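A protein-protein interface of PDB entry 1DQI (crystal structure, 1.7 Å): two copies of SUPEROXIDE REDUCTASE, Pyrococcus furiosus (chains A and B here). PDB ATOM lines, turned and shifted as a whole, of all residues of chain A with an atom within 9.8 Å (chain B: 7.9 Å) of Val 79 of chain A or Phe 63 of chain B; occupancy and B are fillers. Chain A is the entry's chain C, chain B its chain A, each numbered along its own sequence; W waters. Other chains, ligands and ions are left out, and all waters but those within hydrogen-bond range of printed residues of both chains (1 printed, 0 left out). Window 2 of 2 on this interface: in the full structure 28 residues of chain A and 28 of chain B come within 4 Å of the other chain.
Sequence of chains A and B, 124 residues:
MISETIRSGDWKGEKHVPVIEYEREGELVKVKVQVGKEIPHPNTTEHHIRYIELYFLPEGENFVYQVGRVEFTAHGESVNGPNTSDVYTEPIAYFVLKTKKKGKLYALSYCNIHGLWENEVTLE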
ATOM      1  N   THR A  45      16.615 -12.308  30.767  1.00  0.00           N
ATOM      2  CA  THR A  45      16.856 -10.923  31.131  1.00  0.00           C
ATOM      3  C   THR A  45      16.358 -10.665  32.554  1.00  0.00           C
ATOM      4  O   THR A  45      16.943  -9.879  33.298  1.00  0.00           O
ATOM      5  CB  THR A  45      16.134  -9.981  30.150  1.00  0.00           C
ATOM      6  OG1 THR A  45      16.715 -10.126  28.849  1.00  0.00           O
ATOM      7  CG2 THR A  45      16.259  -8.529  30.598  1.00  0.00           C
ATOM      8  N   GLY A  76      20.390 -11.690  27.099  1.00  0.00           N
ATOM      9  CA  GLY A  76      19.339 -11.527  26.100  1.00  0.00           C
ATOM     10  C   GLY A  76      18.756 -10.147  25.878  1.00  0.00           C
ATOM     11  O   GLY A  76      18.010  -9.938  24.927  1.00  0.00           O
ATOM     12  N   GLU A  77      19.085  -9.204  26.750  1.00  0.00           N
ATOM     13  CA  GLU A  77      18.559  -7.856  26.608  1.00  0.00           C
ATOM     14  C   GLU A  77      18.959  -7.216  25.282  1.00  0.00           C
ATOM     15  O   GLU A  77      20.064  -7.437  24.789  1.00  0.00           O
ATOM     16  CB  GLU A  77      19.058  -6.980  27.761  1.00  0.00           C
ATOM     17  CG  GLU A  77      20.579  -6.883  27.844  1.00  0.00           C
ATOM     18  CD  GLU A  77      21.223  -8.116  28.463  1.00  0.00           C
ATOM     19  OE1 GLU A  77      20.535  -8.837  29.220  1.00  0.00           O
ATOM     20  OE2 GLU A  77      22.422  -8.361  28.190  1.00  0.00           O
ATOM     21  N   SER A  78      18.059  -6.416  24.713  1.00  0.00           N
ATOM     22  CA  SER A  78      18.342  -5.709  23.463  1.00  0.00           C
ATOM     23  C   SER A  78      17.326  -4.592  23.268  1.00  0.00           C
ATOM     24  O   SER A  78      16.323  -4.525  23.981  1.00  0.00           O
ATOM     25  CB  SER A  78      18.304  -6.673  22.271  1.00  0.00           C
ATOM     26  OG  SER A  78      17.103  -6.551  21.523  1.00  0.00           O
ATOM     27  N   VAL A  79      17.590  -3.706  22.316  1.00  0.00           N
ATOM     28  CA  VAL A  79      16.677  -2.598  22.055  1.00  0.00           C
ATOM     29  C   VAL A  79      15.333  -3.127  21.571  1.00  0.00           C
ATOM     30  O   VAL A  79      14.344  -2.400  21.545  1.00  0.00           O
ATOM     31  CB  VAL A  79      17.237  -1.635  20.983  1.00  0.00           C
ATOM     32  CG1 VAL A  79      18.478  -0.941  21.506  1.00  0.00           C
ATOM     33  CG2 VAL A  79      17.548  -2.396  19.703  1.00  0.00           C
ATOM     34  N   ASN A  80      15.303  -4.399  21.188  1.00  0.00           N
ATOM     35  CA  ASN A  80      14.067  -5.004  20.714  1.00  0.00           C
ATOM     36  C   ASN A  80      13.347  -5.772  21.816  1.00  0.00           C
ATOM     37  O   ASN A  80      12.454  -6.579  21.546  1.00  0.00           O
ATOM     38  CB  ASN A  80      14.353  -5.915  19.519  1.00  0.00           C
ATOM     39  CG  ASN A  80      14.496  -5.134  18.227  1.00  0.00           C
ATOM     40  OD1 ASN A  80      14.026  -4.000  18.119  1.00  0.00           O
ATOM     41  ND2 ASN A  80      15.149  -5.734  17.240  1.00  0.00           N
ATOM     42  N   GLY A  81      13.751  -5.526  23.060  1.00  0.00           N
ATOM     43  CA  GLY A  81      13.099  -6.169  24.183  1.00  0.00           C
ATOM     44  C   GLY A  81      13.888  -7.190  24.979  1.00  0.00           C
ATOM     45  O   GLY A  81      14.982  -7.600  24.586  1.00  0.00           O
ATOM     46  N   PRO A  82      13.343  -7.619  26.124  1.00  0.00           N
ATOM     47  CA  PRO A  82      14.043  -8.609  26.943  1.00  0.00           C
ATOM     48  C   PRO A  82      14.061  -9.951  26.219  1.00  0.00           C
ATOM     49  O   PRO A  82      13.101 -10.298  25.528  1.00  0.00           O
ATOM     50  CB  PRO A  82      13.219  -8.664  28.228  1.00  0.00           C
ATOM     51  CG  PRO A  82      11.839  -8.230  27.807  1.00  0.00           C
ATOM     52  CD  PRO A  82      12.052  -7.219  26.713  1.00  0.00           C
ATOM     53  N   ASN A  83      15.159 -10.686  26.366  1.00  0.00           N
ATOM     54  CA  ASN A  83      15.309 -12.006  25.752  1.00  0.00           C
ATOM     55  C   ASN A  83      15.202 -12.012  24.225  1.00  0.00           C
ATOM     56  O   ASN A  83      14.602 -12.922  23.650  1.00  0.00           O
ATOM     57  CB  ASN A  83      14.272 -12.965  26.347  1.00  0.00           C
ATOM     58  CG  ASN A  83      14.302 -12.984  27.868  1.00  0.00           C
ATOM     59  OD1 ASN A  83      13.298 -12.699  28.532  1.00  0.00           O
ATOM     60  ND2 ASN A  83      15.456 -13.314  28.426  1.00  0.00           N
ATOM     61  N   THR A  84      15.793 -11.014  23.573  1.00  0.00           N
ATOM     62  CA  THR A  84      15.738 -10.923  22.111  1.00  0.00           C
ATOM     63  C   THR A  84      17.092 -10.809  21.412  1.00  0.00           C
ATOM     64  O   THR A  84      17.172 -10.893  20.189  1.00  0.00           O
ATOM     65  CB  THR A  84      14.894  -9.717  21.671  1.00  0.00           C
ATOM     66  OG1 THR A  84      15.469  -8.515  22.204  1.00  0.00           O
ATOM     67  CG2 THR A  84      13.463  -9.859  22.170  1.00  0.00           C
ATOM     68  N   SER A  85      18.162 -10.621  22.175  1.00  0.00           N
ATOM     69  CA  SER A  85      19.484 -10.473  21.570  1.00  0.00           C
ATOM     70  C   SER A  85      20.129 -11.766  21.081  1.00  0.00           C
ATOM     71  O   SER A  85      21.023 -11.726  20.242  1.00  0.00           O
ATOM     72  CB  SER A  85      20.434  -9.814  22.563  1.00  0.00           C
ATOM     73  OG  SER A  85      20.844 -10.763  23.529  1.00  0.00           O
ATOM     74  N   ASP A  86      19.674 -12.896  21.608  1.00  0.00           N
ATOM     75  CA  ASP A  86      20.233 -14.206  21.276  1.00  0.00           C
ATOM     76  C   ASP A  86      21.686 -14.278  21.729  1.00  0.00           C
ATOM     77  O   ASP A  86      22.488 -15.022  21.169  1.00  0.00           O
ATOM     78  CB  ASP A  86      20.160 -14.497  19.774  1.00  0.00           C
ATOM     79  CG  ASP A  86      20.473 -15.951  19.454  1.00  0.00           C
ATOM     80  OD1 ASP A  86      21.210 -16.211  18.478  1.00  0.00           O
ATOM     81  OD2 ASP A  86      19.984 -16.837  20.186  1.00  0.00           O
ATOM     82  N   VAL A  87      22.021 -13.482  22.738  1.00  0.00           N
ATOM     83  CA  VAL A  87      23.368 -13.466  23.297  1.00  0.00           C
ATOM     84  C   VAL A  87      23.239 -13.663  24.805  1.00  0.00           C
ATOM     85  O   VAL A  87      22.729 -12.794  25.516  1.00  0.00           O
ATOM     86  CB  VAL A  87      24.086 -12.135  23.009  1.00  0.00           C
ATOM     87  CG1 VAL A  87      25.479 -12.153  23.623  1.00  0.00           C
ATOM     88  CG2 VAL A  87      24.177 -11.909  21.503  1.00  0.00           C
ATOM     89  N   PHE B  56      31.002  -8.612  22.261  1.00  0.00           N
ATOM     90  CA  PHE B  56      30.515  -9.192  21.014  1.00  0.00           C
ATOM     91  C   PHE B  56      29.589  -8.217  20.300  1.00  0.00           C
ATOM     92  O   PHE B  56      28.608  -7.751  20.874  1.00  0.00           O
ATOM     93  CB  PHE B  56      29.765 -10.501  21.306  1.00  0.00           C
ATOM     94  CG  PHE B  56      29.087 -11.111  20.100  1.00  0.00           C
ATOM     95  CD1 PHE B  56      29.720 -11.150  18.862  1.00  0.00           C
ATOM     96  CD2 PHE B  56      27.819 -11.676  20.218  1.00  0.00           C
ATOM     97  CE1 PHE B  56      29.101 -11.745  17.758  1.00  0.00           C
ATOM     98  CE2 PHE B  56      27.192 -12.274  19.121  1.00  0.00           C
ATOM     99  CZ  PHE B  56      27.837 -12.308  17.890  1.00  0.00           C
ATOM    100  N   LEU B  57      29.925  -7.888  19.056  1.00  0.00           N
ATOM    101  CA  LEU B  57      29.092  -7.001  18.250  1.00  0.00           C
ATOM    102  C   LEU B  57      28.555  -7.846  17.106  1.00  0.00           C
ATOM    103  O   LEU B  57      29.284  -8.169  16.167  1.00  0.00           O
ATOM    104  CB  LEU B  57      29.906  -5.833  17.682  1.00  0.00           C
ATOM    105  CG  LEU B  57      29.117  -4.910  16.744  1.00  0.00           C
ATOM    106  CD1 LEU B  57      27.964  -4.263  17.505  1.00  0.00           C
ATOM    107  CD2 LEU B  57      30.038  -3.846  16.173  1.00  0.00           C
ATOM    108  N   PRO B  58      27.275  -8.247  17.182  1.00  0.00           N
ATOM    109  CA  PRO B  58      26.683  -9.065  16.118  1.00  0.00           C
ATOM    110  C   PRO B  58      26.737  -8.373  14.764  1.00  0.00           C
ATOM    111  O   PRO B  58      26.588  -7.154  14.672  1.00  0.00           O
ATOM    112  CB  PRO B  58      25.246  -9.296  16.590  1.00  0.00           C
ATOM    113  CG  PRO B  58      25.289  -9.051  18.076  1.00  0.00           C
ATOM    114  CD  PRO B  58      26.317  -7.981  18.270  1.00  0.00           C
ATOM    115  N   GLY B  60      26.028  -6.572  11.542  1.00  0.00           N
ATOM    116  CA  GLY B  60      24.939  -5.701  11.142  1.00  0.00           C
ATOM    117  C   GLY B  60      24.210  -4.976  12.258  1.00  0.00           C
ATOM    118  O   GLY B  60      23.277  -4.223  11.991  1.00  0.00           O
ATOM    119  N   GLU B  61      24.619  -5.190  13.504  1.00  0.00           N
ATOM    120  CA  GLU B  61      23.959  -4.526  14.624  1.00  0.00           C
ATOM    121  C   GLU B  61      24.710  -3.269  15.055  1.00  0.00           C
ATOM    122  O   GLU B  61      25.876  -3.084  14.705  1.00  0.00           O
ATOM    123  CB  GLU B  61      23.797  -5.511  15.785  1.00  0.00           C
ATOM    124  CG  GLU B  61      23.045  -6.771  15.366  1.00  0.00           C
ATOM    125  CD  GLU B  61      22.432  -7.523  16.527  1.00  0.00           C
ATOM    126  OE1 GLU B  61      22.618  -7.093  17.687  1.00  0.00           O
ATOM    127  OE2 GLU B  61      21.762  -8.548  16.275  1.00  0.00           O
ATOM    128  N   ASN B  62      24.040  -2.403  15.812  1.00  0.00           N
ATOM    129  CA  ASN B  62      24.637  -1.140  16.244  1.00  0.00           C
ATOM    130  C   ASN B  62      25.156  -1.064  17.673  1.00  0.00           C
ATOM    131  O   ASN B  62      25.844  -0.107  18.027  1.00  0.00           O
ATOM    132  CB  ASN B  62      23.634  -0.001  16.055  1.00  0.00           C
ATOM    133  CG  ASN B  62      23.328   0.277  14.599  1.00  0.00           C
ATOM    134  OD1 ASN B  62      24.192   0.144  13.732  1.00  0.00           O
ATOM    135  ND2 ASN B  62      22.090   0.669  14.322  1.00  0.00           N
ATOM    136  N   PHE B  63      24.837  -2.052  18.499  1.00  0.00           N
ATOM    137  CA  PHE B  63      25.276  -1.998  19.886  1.00  0.00           C
ATOM    138  C   PHE B  63      26.040  -3.218  20.368  1.00  0.00           C
ATOM    139  O   PHE B  63      25.539  -4.340  20.347  1.00  0.00           O
ATOM    140  CB  PHE B  63      24.064  -1.732  20.780  1.00  0.00           C
ATOM    141  CG  PHE B  63      23.296  -0.499  20.388  1.00  0.00           C
ATOM    142  CD1 PHE B  63      22.015  -0.598  19.852  1.00  0.00           C
ATOM    143  CD2 PHE B  63      23.865   0.763  20.534  1.00  0.00           C
ATOM    144  CE1 PHE B  63      21.310   0.547  19.465  1.00  0.00           C
ATOM    145  CE2 PHE B  63      23.171   1.912  20.152  1.00  0.00           C
ATOM    146  CZ  PHE B  63      21.891   1.802  19.617  1.00  0.00           C
ATOM    147  N   VAL B  64      27.269  -2.981  20.811  1.00  0.00           N
ATOM    148  CA  VAL B  64      28.117  -4.055  21.294  1.00  0.00           C
ATOM    149  C   VAL B  64      27.589  -4.574  22.621  1.00  0.00           C
ATOM    150  O   VAL B  64      26.995  -3.828  23.402  1.00  0.00           O
ATOM    151  CB  VAL B  64      29.577  -3.573  21.477  1.00  0.00           C
ATOM    152  CG1 VAL B  64      29.672  -2.629  22.668  1.00  0.00           C
ATOM    153  CG2 VAL B  64      30.504  -4.768  21.659  1.00  0.00           C
ATOM    154  N   TYR B  65      27.799  -5.860  22.862  1.00  0.00           N
ATOM    155  CA  TYR B  65      27.366  -6.477  24.103  1.00  0.00           C
ATOM    156  C   TYR B  65      28.571  -6.958  24.879  1.00  0.00           C
ATOM    157  O   TYR B  65      29.500  -7.529  24.306  1.00  0.00           O
ATOM    158  CB  TYR B  65      26.473  -7.685  23.831  1.00  0.00           C
ATOM    159  CG  TYR B  65      25.141  -7.334  23.234  1.00  0.00           C
ATOM    160  CD1 TYR B  65      24.763  -7.835  21.990  1.00  0.00           C
ATOM    161  CD2 TYR B  65      24.256  -6.501  23.910  1.00  0.00           C
ATOM    162  CE1 TYR B  65      23.534  -7.513  21.435  1.00  0.00           C
ATOM    163  CE2 TYR B  65      23.023  -6.171  23.364  1.00  0.00           C
ATOM    164  CZ  TYR B  65      22.670  -6.680  22.127  1.00  0.00           C
ATOM    165  OH  TYR B  65      21.449  -6.355  21.590  1.00  0.00           O
ATOM    166  N   GLN B  66      28.569  -6.717  26.184  1.00  0.00           N
ATOM    167  CA  GLN B  66      29.657  -7.214  27.006  1.00  0.00           C
ATOM    168  C   GLN B  66      29.254  -8.649  27.318  1.00  0.00           C
ATOM    169  O   GLN B  66      28.169  -8.892  27.845  1.00  0.00           O
ATOM    170  CB  GLN B  66      29.783  -6.419  28.306  1.00  0.00           C
ATOM    171  CG  GLN B  66      30.988  -6.848  29.135  1.00  0.00           C
ATOM    172  CD  GLN B  66      31.288  -5.895  30.273  1.00  0.00           C
ATOM    173  OE1 GLN B  66      32.259  -5.132  30.225  1.00  0.00           O
ATOM    174  NE2 GLN B  66      30.460  -5.933  31.305  1.00  0.00           N
HETATM  175  O   HOH W   1      20.485  -3.763  21.785  1.00  0.00           O
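The side-chain hydroxyl (OG) of Ser 78 of chain A lies within hydrogen-bond range of the backbone NH (N) of Asn 80 of chain A (2.8 Å). The side-chain hydroxyl (OG1) of Thr 45 of chain A sits at hydrogen-bond distance from the backbone NH (N) of Glu 77 of chain A (3.3 Å). O of Tyr 65 of chain B sits at hydrogen-bond distance from N of Phe 56 of chain B, at 2.8 Å. OG of Ser 85 of chain A lies close to N of Val 87 of chain A (3.1 Å). The backbone NH of Gly 76 of chain A sits at hydrogen-bond distance from the backbone carbonyl oxygen of Val 87 of chain A, 3.0 Å away. The side-chain hydroxyl (OG) of Ser 78 of chain A is in hydrogen-bond range of the side-chain hydroxyl (OG1) of Thr 84 of chain A.
Among the printed residues, pairs that only touch across the chains: Ser 78 of chain A with Tyr 65 of chain B, Glu 77 of chain A with Tyr 65 of chain B, Ser 85 of chain A with Tyr 65 of chain B, Val 79 of chain A with Phe 63 of chain B and Val 87 of chain A with Phe 56 of chain B.
Of the printed residues of chain B, Glu 77 of chain A touches Tyr 65. Ser 78 of chain A touches just one residue of chain B: Tyr 65 (3.2 Å). Val 79 of chain A touches one residue of chain B. Of the printed residues of chain B, Ser 85 of chain A touches Tyr 65. Printed residues of chain B within 4 Å of Val 87 of chain A: Phe 56. Printed residues of chain A within 4 Å of Phe 56 of chain B: Val 87 (3.9 Å). Phe 63 of chain B touches just one residue of chain A: Val 79. No residue of chain A comes within 4 Å of Val 64 of chain B. Of the printed residues of chain A, Tyr 65 of chain B touches Glu 77 (3.5 Å), Ser 78 (3.2 Å) and Ser 85 (3.7 Å). The nearest printed residue of chain B that does not touch Ser 85 of chain A is Glu 61 of chain B (5.1 Å).
Of the 10 printed residues of chain B, 3 touch a printed residue of chain A. Of the 13 printed residues of chain A, 5 touch a printed residue of chain B. Hydrophobic or aromatic side chains of chain A that line the printed part of chain B: Val 79 and Val 87. Among the printed residues, 5 pairs touch across the chains.
No position is printed for both chains. Of the 5 pairs that touch across the chains among the printed residues, none has its exchanged pair printed and touching as well.
Water W1 lies within hydrogen-bond range of OH of Tyr 65 of chain B (2.8 Å) and N of Val 79 of chain A (2.9 Å).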
